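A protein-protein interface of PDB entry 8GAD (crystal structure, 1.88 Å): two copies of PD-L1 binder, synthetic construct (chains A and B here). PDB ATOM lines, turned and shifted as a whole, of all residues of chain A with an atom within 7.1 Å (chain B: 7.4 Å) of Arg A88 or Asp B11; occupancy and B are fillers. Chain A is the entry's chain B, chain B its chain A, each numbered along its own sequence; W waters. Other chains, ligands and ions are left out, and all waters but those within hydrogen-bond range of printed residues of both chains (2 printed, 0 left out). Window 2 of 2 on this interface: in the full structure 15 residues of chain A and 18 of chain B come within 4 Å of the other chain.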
ATOM      1  N   ALA A  82     -18.198 -13.265 -35.296  1.00  0.00           N
ATOM      2  CA  ALA A  82     -18.334 -12.103 -34.424  1.00  0.00           C
ATOM      3  C   ALA A  82     -16.991 -11.678 -33.838  1.00  0.00           C
ATOM      4  O   ALA A  82     -16.699 -10.479 -33.747  1.00  0.00           O
ATOM      5  CB  ALA A  82     -19.324 -12.406 -33.301  1.00  0.00           C
ATOM      6  N   GLU A  83     -16.172 -12.644 -33.400  1.00  0.00           N
ATOM      7  CA  GLU A  83     -14.858 -12.289 -32.863  1.00  0.00           C
ATOM      8  C   GLU A  83     -13.952 -11.758 -33.959  1.00  0.00           C
ATOM      9  O   GLU A  83     -13.189 -10.810 -33.741  1.00  0.00           O
ATOM     10  CB  GLU A  83     -14.199 -13.485 -32.168  1.00  0.00           C
ATOM     11  CG  GLU A  83     -14.983 -14.054 -30.989  1.00  0.00           C
ATOM     12  CD  GLU A  83     -14.436 -15.391 -30.506  1.00  0.00           C
ATOM     13  OE1 GLU A  83     -15.245 -16.244 -30.058  1.00  0.00           O
ATOM     14  OE2 GLU A  83     -13.200 -15.585 -30.568  1.00  0.00           O
ATOM     15  N   GLU A  85     -14.819 -10.067 -36.520  1.00  0.00           N
ATOM     16  CA  GLU A  85     -15.255  -8.728 -36.886  1.00  0.00           C
ATOM     17  C   GLU A  85     -15.329  -7.781 -35.701  1.00  0.00           C
ATOM     18  O   GLU A  85     -15.706  -6.619 -35.880  1.00  0.00           O
ATOM     19  CB  GLU A  85     -16.609  -8.817 -37.604  1.00  0.00           C
ATOM     20  CG  GLU A  85     -16.505  -9.702 -38.860  1.00  0.00           C
ATOM     21  CD  GLU A  85     -17.787  -9.785 -39.674  1.00  0.00           C
ATOM     22  OE1 GLU A  85     -18.862  -9.412 -39.156  1.00  0.00           O
ATOM     23  OE2 GLU A  85     -17.706 -10.238 -40.841  1.00  0.00           O
ATOM     24  N   GLY A  86     -14.987  -8.251 -34.501  1.00  0.00           N
ATOM     25  CA  GLY A  86     -15.027  -7.419 -33.311  1.00  0.00           C
ATOM     26  C   GLY A  86     -16.404  -6.928 -32.925  1.00  0.00           C
ATOM     27  O   GLY A  86     -16.525  -5.830 -32.375  1.00  0.00           O
ATOM     28  N   ASN A  87     -17.457  -7.693 -33.211  1.00  0.00           N
ATOM     29  CA  ASN A  87     -18.819  -7.277 -32.866  1.00  0.00           C
ATOM     30  C   ASN A  87     -19.210  -8.011 -31.585  1.00  0.00           C
ATOM     31  O   ASN A  87     -19.618  -9.179 -31.610  1.00  0.00           O
ATOM     32  CB  ASN A  87     -19.803  -7.539 -34.008  1.00  0.00           C
ATOM     33  CG  ASN A  87     -21.191  -6.956 -33.728  1.00  0.00           C
ATOM     34  OD1 ASN A  87     -21.646  -6.927 -32.581  1.00  0.00           O
ATOM     35  ND2 ASN A  87     -21.863  -6.487 -34.774  1.00  0.00           N
ATOM     36  N   ARG A  88     -19.069  -7.321 -30.458  1.00  0.00           N
ATOM     37  CA  ARG A  88     -19.386  -7.912 -29.169  1.00  0.00           C
ATOM     38  C   ARG A  88     -20.879  -8.171 -29.004  1.00  0.00           C
ATOM     39  O   ARG A  88     -21.271  -8.992 -28.168  1.00  0.00           O
ATOM     40  CB  ARG A  88     -18.871  -6.979 -28.072  1.00  0.00           C
ATOM     41  CG  ARG A  88     -17.348  -6.896 -28.019  1.00  0.00           C
ATOM     42  CD  ARG A  88     -16.874  -5.730 -27.157  1.00  0.00           C
ATOM     43  NE  ARG A  88     -17.295  -4.421 -27.663  1.00  0.00           N
ATOM     44  CZ  ARG A  88     -16.968  -3.270 -27.084  1.00  0.00           C
ATOM     45  NH1 ARG A  88     -16.244  -3.240 -25.982  1.00  0.00           N
ATOM     46  NH2 ARG A  88     -17.371  -2.121 -27.629  1.00  0.00           N
ATOM     47  N   PHE A  89     -21.723  -7.495 -29.782  1.00  0.00           N
ATOM     48  CA  PHE A  89     -23.159  -7.675 -29.616  1.00  0.00           C
ATOM     49  C   PHE A  89     -23.650  -8.953 -30.278  1.00  0.00           C
ATOM     50  O   PHE A  89     -24.479  -9.669 -29.703  1.00  0.00           O
ATOM     51  CB  PHE A  89     -23.890  -6.466 -30.189  1.00  0.00           C
ATOM     52  CG  PHE A  89     -23.454  -5.178 -29.573  1.00  0.00           C
ATOM     53  CD1 PHE A  89     -23.885  -4.820 -28.306  1.00  0.00           C
ATOM     54  CD2 PHE A  89     -22.586  -4.336 -30.248  1.00  0.00           C
ATOM     55  CE1 PHE A  89     -23.485  -3.646 -27.733  1.00  0.00           C
ATOM     56  CE2 PHE A  89     -22.166  -3.150 -29.667  1.00  0.00           C
ATOM     57  CZ  PHE A  89     -22.612  -2.805 -28.411  1.00  0.00           C
ATOM     58  N   ILE A  90     -23.172  -9.242 -31.493  1.00  0.00           N
ATOM     59  CA  ILE A  90     -23.438 -10.548 -32.094  1.00  0.00           C
ATOM     60  C   ILE A  90     -22.922 -11.649 -31.185  1.00  0.00           C
ATOM     61  O   ILE A  90     -23.593 -12.668 -30.977  1.00  0.00           O
ATOM     62  CB  ILE A  90     -22.820 -10.631 -33.499  1.00  0.00           C
ATOM     63  CG1 ILE A  90     -23.489  -9.611 -34.426  1.00  0.00           C
ATOM     64  CG2 ILE A  90     -22.914 -12.061 -34.058  1.00  0.00           C
ATOM     65  CD1 ILE A  90     -22.861  -9.565 -35.817  1.00  0.00           C
ATOM     66  N   GLU A  91     -21.735 -11.451 -30.611  1.00  0.00           N
ATOM     67  CA  GLU A  91     -21.214 -12.407 -29.641  1.00  0.00           C
ATOM     68  C   GLU A  91     -22.210 -12.629 -28.504  1.00  0.00           C
ATOM     69  O   GLU A  91     -22.499 -13.772 -28.132  1.00  0.00           O
ATOM     70  CB  GLU A  91     -19.873 -11.897 -29.112  1.00  0.00           C
ATOM     71  CG  GLU A  91     -19.148 -12.844 -28.232  1.00  0.00           C
ATOM     72  CD  GLU A  91     -17.809 -12.272 -27.798  1.00  0.00           C
ATOM     73  OE1 GLU A  91     -17.194 -11.525 -28.594  1.00  0.00           O
ATOM     74  OE2 GLU A  91     -17.379 -12.554 -26.661  1.00  0.00           O
ATOM     75  N   ALA A  92     -22.745 -11.545 -27.931  1.00  0.00           N
ATOM     76  CA  ALA A  92     -23.695 -11.699 -26.827  1.00  0.00           C
ATOM     77  C   ALA A  92     -24.988 -12.385 -27.277  1.00  0.00           C
ATOM     78  O   ALA A  92     -25.552 -13.208 -26.535  1.00  0.00           O
ATOM     79  CB  ALA A  92     -23.998 -10.331 -26.202  1.00  0.00           C
ATOM     80  N   MET A  93     -25.513 -12.015 -28.446  1.00  0.00           N
ATOM     81  CA  MET A  93     -26.659 -12.743 -28.998  1.00  0.00           C
ATOM     82  C   MET A  93     -26.380 -14.225 -29.118  1.00  0.00           C
ATOM     83  O   MET A  93     -27.245 -15.058 -28.823  1.00  0.00           O
ATOM     84  CB  MET A  93     -27.062 -12.176 -30.361  1.00  0.00           C
ATOM     85  CG  MET A  93     -28.490 -12.533 -30.828  1.00  0.00           C
ATOM     86  SD  MET A  93     -29.838 -12.535 -29.638  1.00  0.00           S
ATOM     87  CE  MET A  93     -29.999 -10.748 -29.350  1.00  0.00           C
ATOM     88  N   GLY A  94     -25.199 -14.571 -29.620  1.00  0.00           N
ATOM     89  CA  GLY A  94     -24.828 -15.969 -29.692  1.00  0.00           C
ATOM     90  C   GLY A  94     -24.935 -16.655 -28.350  1.00  0.00           C
ATOM     91  O   GLY A  94     -25.466 -17.762 -28.251  1.00  0.00           O
ATOM     92  N   GLU B   4     -21.854   5.074 -32.366  1.00  0.00           N
ATOM     93  CA  GLU B   4     -20.692   5.517 -31.599  1.00  0.00           C
ATOM     94  C   GLU B   4     -21.006   5.563 -30.105  1.00  0.00           C
ATOM     95  O   GLU B   4     -20.234   5.065 -29.277  1.00  0.00           O
ATOM     96  CB  GLU B   4     -20.244   6.902 -32.089  1.00  0.00           C
ATOM     97  CG  GLU B   4     -19.598   6.995 -33.475  1.00  0.00           C
ATOM     98  CD  GLU B   4     -20.562   6.778 -34.661  1.00  0.00           C
ATOM     99  OE1 GLU B   4     -21.802   6.904 -34.499  1.00  0.00           O
ATOM    100  OE2 GLU B   4     -20.061   6.567 -35.791  1.00  0.00           O
ATOM    101  N   GLU B   5     -22.145   6.166 -29.742  1.00  0.00           N
ATOM    102  CA  GLU B   5     -22.533   6.262 -28.333  1.00  0.00           C
ATOM    103  C   GLU B   5     -22.728   4.884 -27.703  1.00  0.00           C
ATOM    104  O   GLU B   5     -22.377   4.668 -26.536  1.00  0.00           O
ATOM    105  CB  GLU B   5     -23.818   7.078 -28.206  1.00  0.00           C
ATOM    106  CG  GLU B   5     -23.695   8.553 -28.564  1.00  0.00           C
ATOM    107  CD  GLU B   5     -25.047   9.270 -28.603  1.00  0.00           C
ATOM    108  OE1 GLU B   5     -25.955   8.809 -29.333  1.00  0.00           O
ATOM    109  OE2 GLU B   5     -25.194  10.309 -27.927  1.00  0.00           O
ATOM    110  N   ILE B   6     -23.311   3.947 -28.454  1.00  0.00           N
ATOM    111  CA  ILE B   6     -23.493   2.585 -27.957  1.00  0.00           C
ATOM    112  C   ILE B   6     -22.144   1.929 -27.682  1.00  0.00           C
ATOM    113  O   ILE B   6     -21.941   1.306 -26.630  1.00  0.00           O
ATOM    114  CB  ILE B   6     -24.337   1.770 -28.954  1.00  0.00           C
ATOM    115  CG1 ILE B   6     -25.800   2.239 -28.934  1.00  0.00           C
ATOM    116  CG2 ILE B   6     -24.232   0.287 -28.680  1.00  0.00           C
ATOM    117  CD1 ILE B   6     -26.644   1.686 -30.139  1.00  0.00           C
ATOM    118  N   GLU B   7     -21.203   2.052 -28.625  1.00  0.00           N
ATOM    119  CA  GLU B   7     -19.879   1.467 -28.424  1.00  0.00           C
ATOM    120  C   GLU B   7     -19.205   2.074 -27.208  1.00  0.00           C
ATOM    121  O   GLU B   7     -18.558   1.364 -26.432  1.00  0.00           O
ATOM    122  CB  GLU B   7     -18.987   1.669 -29.655  1.00  0.00           C
ATOM    123  CG  GLU B   7     -19.408   0.862 -30.875  1.00  0.00           C
ATOM    124  CD  GLU B   7     -19.144  -0.642 -30.738  1.00  0.00           C
ATOM    125  OE1 GLU B   7     -18.237  -1.040 -29.970  1.00  0.00           O
ATOM    126  OE2 GLU B   7     -19.839  -1.427 -31.430  1.00  0.00           O
ATOM    127  N   GLU B   8     -19.334   3.392 -27.037  1.00  0.00           N
ATOM    128  CA  GLU B   8     -18.768   4.025 -25.850  1.00  0.00           C
ATOM    129  C   GLU B   8     -19.408   3.491 -24.576  1.00  0.00           C
ATOM    130  O   GLU B   8     -18.710   3.217 -23.595  1.00  0.00           O
ATOM    131  CB  GLU B   8     -18.919   5.545 -25.916  1.00  0.00           C
ATOM    132  CG  GLU B   8     -18.378   6.216 -24.648  1.00  0.00           C
ATOM    133  CD  GLU B   8     -18.465   7.736 -24.646  1.00  0.00           C
ATOM    134  OE1 GLU B   8     -18.778   8.361 -25.684  1.00  0.00           O
ATOM    135  OE2 GLU B   8     -18.220   8.311 -23.572  1.00  0.00           O
ATOM    136  N   ALA B   9     -20.738   3.339 -24.561  1.00  0.00           N
ATOM    137  CA  ALA B   9     -21.381   2.814 -23.360  1.00  0.00           C
ATOM    138  C   ALA B   9     -20.868   1.421 -23.033  1.00  0.00           C
ATOM    139  O   ALA B   9     -20.617   1.106 -21.866  1.00  0.00           O
ATOM    140  CB  ALA B   9     -22.906   2.803 -23.516  1.00  0.00           C
ATOM    141  N   TYR B  10     -20.711   0.566 -24.050  1.00  0.00           N
ATOM    142  CA  TYR B  10     -20.198  -0.776 -23.799  1.00  0.00           C
ATOM    143  C   TYR B  10     -18.789  -0.691 -23.229  1.00  0.00           C
ATOM    144  O   TYR B  10     -18.460  -1.361 -22.240  1.00  0.00           O
ATOM    145  CB  TYR B  10     -20.196  -1.596 -25.092  1.00  0.00           C
ATOM    146  CG  TYR B  10     -20.041  -3.085 -24.853  1.00  0.00           C
ATOM    147  CD1 TYR B  10     -18.836  -3.632 -24.430  1.00  0.00           C
ATOM    148  CD2 TYR B  10     -21.104  -3.952 -25.071  1.00  0.00           C
ATOM    149  CE1 TYR B  10     -18.706  -4.996 -24.205  1.00  0.00           C
ATOM    150  CE2 TYR B  10     -20.981  -5.322 -24.854  1.00  0.00           C
ATOM    151  CZ  TYR B  10     -19.781  -5.833 -24.416  1.00  0.00           C
ATOM    152  OH  TYR B  10     -19.643  -7.186 -24.196  1.00  0.00           O
ATOM    153  N   ASP B  11     -17.945   0.146 -23.849  1.00  0.00           N
ATOM    154  CA  ASP B  11     -16.578   0.361 -23.360  1.00  0.00           C
ATOM    155  C   ASP B  11     -16.566   0.801 -21.899  1.00  0.00           C
ATOM    156  O   ASP B  11     -15.740   0.331 -21.102  1.00  0.00           O
ATOM    157  CB  ASP B  11     -15.871   1.425 -24.197  1.00  0.00           C
ATOM    158  CG  ASP B  11     -15.506   0.955 -25.602  1.00  0.00           C
ATOM    159  OD1 ASP B  11     -15.639  -0.249 -25.911  1.00  0.00           O
ATOM    160  OD2 ASP B  11     -15.049   1.816 -26.389  1.00  0.00           O
ATOM    161  N   LEU B  12     -17.441   1.740 -21.534  1.00  0.00           N
ATOM    162  CA  LEU B  12     -17.431   2.239 -20.159  1.00  0.00           C
ATOM    163  C   LEU B  12     -17.840   1.168 -19.165  1.00  0.00           C
ATOM    164  O   LEU B  12     -17.349   1.162 -18.030  1.00  0.00           O
ATOM    165  CB  LEU B  12     -18.353   3.452 -20.028  1.00  0.00           C
ATOM    166  CG  LEU B  12     -17.834   4.701 -20.747  1.00  0.00           C
ATOM    167  CD1 LEU B  12     -18.838   5.801 -20.621  1.00  0.00           C
ATOM    168  CD2 LEU B  12     -16.491   5.134 -20.177  1.00  0.00           C
ATOM    169  N   VAL B  13     -18.751   0.271 -19.553  1.00  0.00           N
ATOM    170  CA  VAL B  13     -19.114  -0.821 -18.659  1.00  0.00           C
ATOM    171  C   VAL B  13     -17.948  -1.782 -18.491  1.00  0.00           C
ATOM    172  O   VAL B  13     -17.659  -2.234 -17.373  1.00  0.00           O
ATOM    173  CB  VAL B  13     -20.378  -1.538 -19.167  1.00  0.00           C
ATOM    174  CG1 VAL B  13     -20.685  -2.751 -18.300  1.00  0.00           C
ATOM    175  CG2 VAL B  13     -21.574  -0.569 -19.177  1.00  0.00           C
ATOM    176  N   GLU B  14     -17.267  -2.133 -19.590  1.00  0.00           N
ATOM    177  CA  GLU B  14     -16.059  -2.945 -19.459  1.00  0.00           C
ATOM    178  C   GLU B  14     -15.026  -2.246 -18.586  1.00  0.00           C
ATOM    179  O   GLU B  14     -14.374  -2.888 -17.753  1.00  0.00           O
ATOM    180  CB  GLU B  14     -15.431  -3.249 -20.822  1.00  0.00           C
ATOM    181  CG  GLU B  14     -16.184  -4.163 -21.764  1.00  0.00           C
ATOM    182  CD  GLU B  14     -15.377  -4.378 -23.045  1.00  0.00           C
ATOM    183  OE1 GLU B  14     -14.308  -3.735 -23.167  1.00  0.00           O
ATOM    184  OE2 GLU B  14     -15.772  -5.189 -23.913  1.00  0.00           O
ATOM    185  N   GLU B  15     -14.832  -0.933 -18.785  1.00  0.00           N
ATOM    186  CA  GLU B  15     -13.855  -0.213 -17.956  1.00  0.00           C
ATOM    187  C   GLU B  15     -14.273  -0.198 -16.490  1.00  0.00           C
ATOM    188  O   GLU B  15     -13.424  -0.320 -15.596  1.00  0.00           O
ATOM    189  CB  GLU B  15     -13.662   1.221 -18.456  1.00  0.00           C
ATOM    190  CG  GLU B  15     -12.511   2.002 -17.744  1.00  0.00           C
ATOM    191  CD  GLU B  15     -11.126   1.472 -18.014  1.00  0.00           C
ATOM    192  OE1 GLU B  15     -10.951   0.693 -18.964  1.00  0.00           O
ATOM    193  OE2 GLU B  15     -10.201   1.827 -17.247  1.00  0.00           O
ATOM    194  N   ALA B  16     -15.574  -0.027 -16.221  1.00  0.00           N
ATOM    195  CA  ALA B  16     -16.053  -0.066 -14.840  1.00  0.00           C
ATOM    196  C   ALA B  16     -15.774  -1.419 -14.200  1.00  0.00           C
ATOM    197  O   ALA B  16     -15.372  -1.499 -13.033  1.00  0.00           O
ATOM    198  CB  ALA B  16     -17.554   0.225 -14.797  1.00  0.00           C
ATOM    199  N   GLU B  17     -15.999  -2.495 -14.951  1.00  0.00           N
ATOM    200  CA  GLU B  17     -15.827  -3.845 -14.424  1.00  0.00           C
ATOM    201  C   GLU B  17     -14.351  -4.195 -14.287  1.00  0.00           C
ATOM    202  O   GLU B  17     -13.973  -4.966 -13.397  1.00  0.00           O
ATOM    203  CB  GLU B  17     -16.586  -4.816 -15.345  1.00  0.00           C
ATOM    204  CG  GLU B  17     -16.068  -6.251 -15.451  1.00  0.00           C
ATOM    205  CD  GLU B  17     -16.802  -7.036 -16.544  1.00  0.00           C
ATOM    206  OE1 GLU B  17     -17.913  -7.552 -16.282  1.00  0.00           O
ATOM    207  OE2 GLU B  17     -16.278  -7.110 -17.680  1.00  0.00           O
ATOM    208  N   LYS B  18     -13.505  -3.596 -15.132  1.00  0.00           N
ATOM    209  CA  LYS B  18     -12.062  -3.792 -15.050  1.00  0.00           C
ATOM    210  C   LYS B  18     -11.470  -3.086 -13.837  1.00  0.00           C
ATOM    211  O   LYS B  18     -10.607  -3.646 -13.146  1.00  0.00           O
ATOM    212  CB  LYS B  18     -11.412  -3.265 -16.331  1.00  0.00           C
ATOM    213  CG  LYS B  18      -9.921  -3.031 -16.255  1.00  0.00           C
ATOM    214  CD  LYS B  18      -9.356  -3.209 -17.642  1.00  0.00           C
ATOM    215  CE  LYS B  18      -8.735  -1.919 -18.131  1.00  0.00           C
ATOM    216  NZ  LYS B  18      -8.704  -1.871 -19.628  1.00  0.00           N
ATOM    217  N   LEU B  24     -18.218   5.011 -13.617  1.00  0.00           N
ATOM    218  CA  LEU B  24     -18.275   4.794 -15.057  1.00  0.00           C
ATOM    219  C   LEU B  24     -19.543   4.047 -15.466  1.00  0.00           C
ATOM    220  O   LEU B  24     -20.027   4.249 -16.584  1.00  0.00           O
ATOM    221  CB  LEU B  24     -17.030   4.038 -15.517  1.00  0.00           C
ATOM    222  CG  LEU B  24     -15.724   4.768 -15.212  1.00  0.00           C
ATOM    223  CD1 LEU B  24     -14.555   3.899 -15.622  1.00  0.00           C
ATOM    224  CD2 LEU B  24     -15.680   6.123 -15.929  1.00  0.00           C
ATOM    225  N   ALA B  28     -22.230   5.323 -18.226  1.00  0.00           N
ATOM    226  CA  ALA B  28     -22.760   4.439 -19.267  1.00  0.00           C
ATOM    227  C   ALA B  28     -24.288   4.469 -19.294  1.00  0.00           C
ATOM    228  O   ALA B  28     -24.895   4.509 -20.370  1.00  0.00           O
ATOM    229  CB  ALA B  28     -22.247   3.007 -19.065  1.00  0.00           C
ATOM    230  N   ILE B  53     -28.543  -5.286 -24.700  1.00  0.00           N
ATOM    231  CA  ILE B  53     -27.430  -6.162 -24.337  1.00  0.00           C
ATOM    232  C   ILE B  53     -26.534  -5.500 -23.300  1.00  0.00           C
ATOM    233  O   ILE B  53     -26.039  -6.160 -22.365  1.00  0.00           O
ATOM    234  CB  ILE B  53     -26.637  -6.543 -25.597  1.00  0.00           C
ATOM    235  CG1 ILE B  53     -27.421  -7.567 -26.430  1.00  0.00           C
ATOM    236  CG2 ILE B  53     -25.261  -7.066 -25.242  1.00  0.00           C
ATOM    237  CD1 ILE B  53     -26.888  -7.689 -27.867  1.00  0.00           C
ATOM    238  N   ILE B  54     -26.293  -4.193 -23.448  1.00  0.00           N
ATOM    239  CA  ILE B  54     -25.447  -3.490 -22.480  1.00  0.00           C
ATOM    240  C   ILE B  54     -26.179  -3.342 -21.147  1.00  0.00           C
ATOM    241  O   ILE B  54     -25.576  -3.480 -20.070  1.00  0.00           O
ATOM    242  CB  ILE B  54     -25.009  -2.119 -23.029  1.00  0.00           C
ATOM    243  CG1 ILE B  54     -24.257  -2.259 -24.358  1.00  0.00           C
ATOM    244  CG2 ILE B  54     -24.101  -1.395 -22.016  1.00  0.00           C
ATOM    245  CD1 ILE B  54     -24.066  -0.892 -25.090  1.00  0.00           C
ATOM    246  N   LYS B  57     -25.788  -6.466 -19.252  1.00  0.00           N
ATOM    247  CA  LYS B  57     -24.455  -6.517 -18.653  1.00  0.00           C
ATOM    248  C   LYS B  57     -24.394  -5.689 -17.371  1.00  0.00           C
ATOM    249  O   LYS B  57     -23.796  -6.112 -16.369  1.00  0.00           O
ATOM    250  CB  LYS B  57     -23.434  -6.033 -19.687  1.00  0.00           C
ATOM    251  CG  LYS B  57     -21.968  -6.300 -19.363  1.00  0.00           C
ATOM    252  CD  LYS B  57     -21.086  -5.854 -20.553  1.00  0.00           C
ATOM    253  CE  LYS B  57     -19.591  -6.018 -20.274  1.00  0.00           C
ATOM    254  NZ  LYS B  57     -19.288  -7.252 -19.485  1.00  0.00           N
HETATM  255  O   HOH W   1     -18.416  -4.410 -30.473  1.00  0.00           O
HETATM  256  O   HOH W   2     -20.385  -9.527 -25.564  1.00  0.00           O
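The side-chain carboxylate of Glu B7 is in salt-bridge range of the guanidinium group of Arg A88, at 2.7 Å.
OD1 of Asp B11 is in salt-bridge range of NH1 of Arg A88, 3.1 Å away.
The guanidinium group of Arg A88 is in salt-bridge range of the side-chain carboxylate of Glu B14 (2.9 Å).
The side-chain amide oxygen (OD1) of Asn A87 lies within hydrogen-bond range of the backbone NH (N) of Phe A89 (2.9 Å).
Among the printed residues, pairs that only touch across the chains: Arg A88 with Tyr B10 (3.0 Å), Phe A89 with Glu B7 (3.4 Å), Phe A89 with Ile B6 (3.5 Å), Phe A89 with Tyr B10 (3.6 Å), Phe A89 with Ile B53 (3.6 Å), Ala A92 with Ile B53 (3.6 Å) and Phe A89 with Ile B54 (3.7 Å).
Printed residues of chain B within 4 Å of Arg A88: Glu B7 (2.7 Å), Tyr B10 (3.0 Å), Asp B11 (3.1 Å) and Glu B14 (2.9 Å).
Of the printed residues of chain A, Asp B11 touches Arg A88.
Printed residues of chain A within 4 Å of Ile B54: Phe A89 (3.7 Å).
Of the printed residues of chain B, Phe A89 touches Ile B6 (3.5 Å), Glu B7 (3.4 Å), Tyr B10 (3.6 Å), Ile B53 (3.6 Å) and Ile B54 (3.7 Å).
Ala B16 touches none of the printed residues of chain A.
The nearest residue of chain B that does not touch Arg A88 is Ile B53 (5.3 Å).
The nearest printed residue of chain A that does not touch Asp B11 is Phe A89 (7.2 Å).
The nearest printed residue of chain B that does not touch Ala A92 is Tyr B10 (5.7 Å).
Hydrophobic or aromatic side chains of chain B within 4 Å of the printed part of chain A: Ile B6, Tyr B10, Ile B53 and Ile B54.
Along chain A the printed residues that touch a printed residue of chain B span positions 88 to 92.
Among the printed residues, 10 pairs touch across the chains.
Among the printed residues, Asp or Glu carboxylates within 4 Å of a Lys or Arg side-chain nitrogen of the other chain: Arg A88 with Glu B7 (2.7 Å), Arg A88 with Asp B11 (3.1 Å) and Arg A88 with Glu B14 (2.9 Å).
No position is printed for both chains.
Of the 10 pairs that touch across the chains among the printed residues, none has its exchanged pair printed and touching as well.
Water W2 lies within hydrogen-bond range of the backbone carbonyl oxygen (O) of Arg A88 (2.8 Å) and the side-chain hydroxyl (OH) of Tyr B10 (2.8 Å).
Water W1 lies within hydrogen-bond range of N of Arg A88 (3.0 Å), O of Gly A86 (3.0 Å) and OE1 of Glu B7 (3.4 Å).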
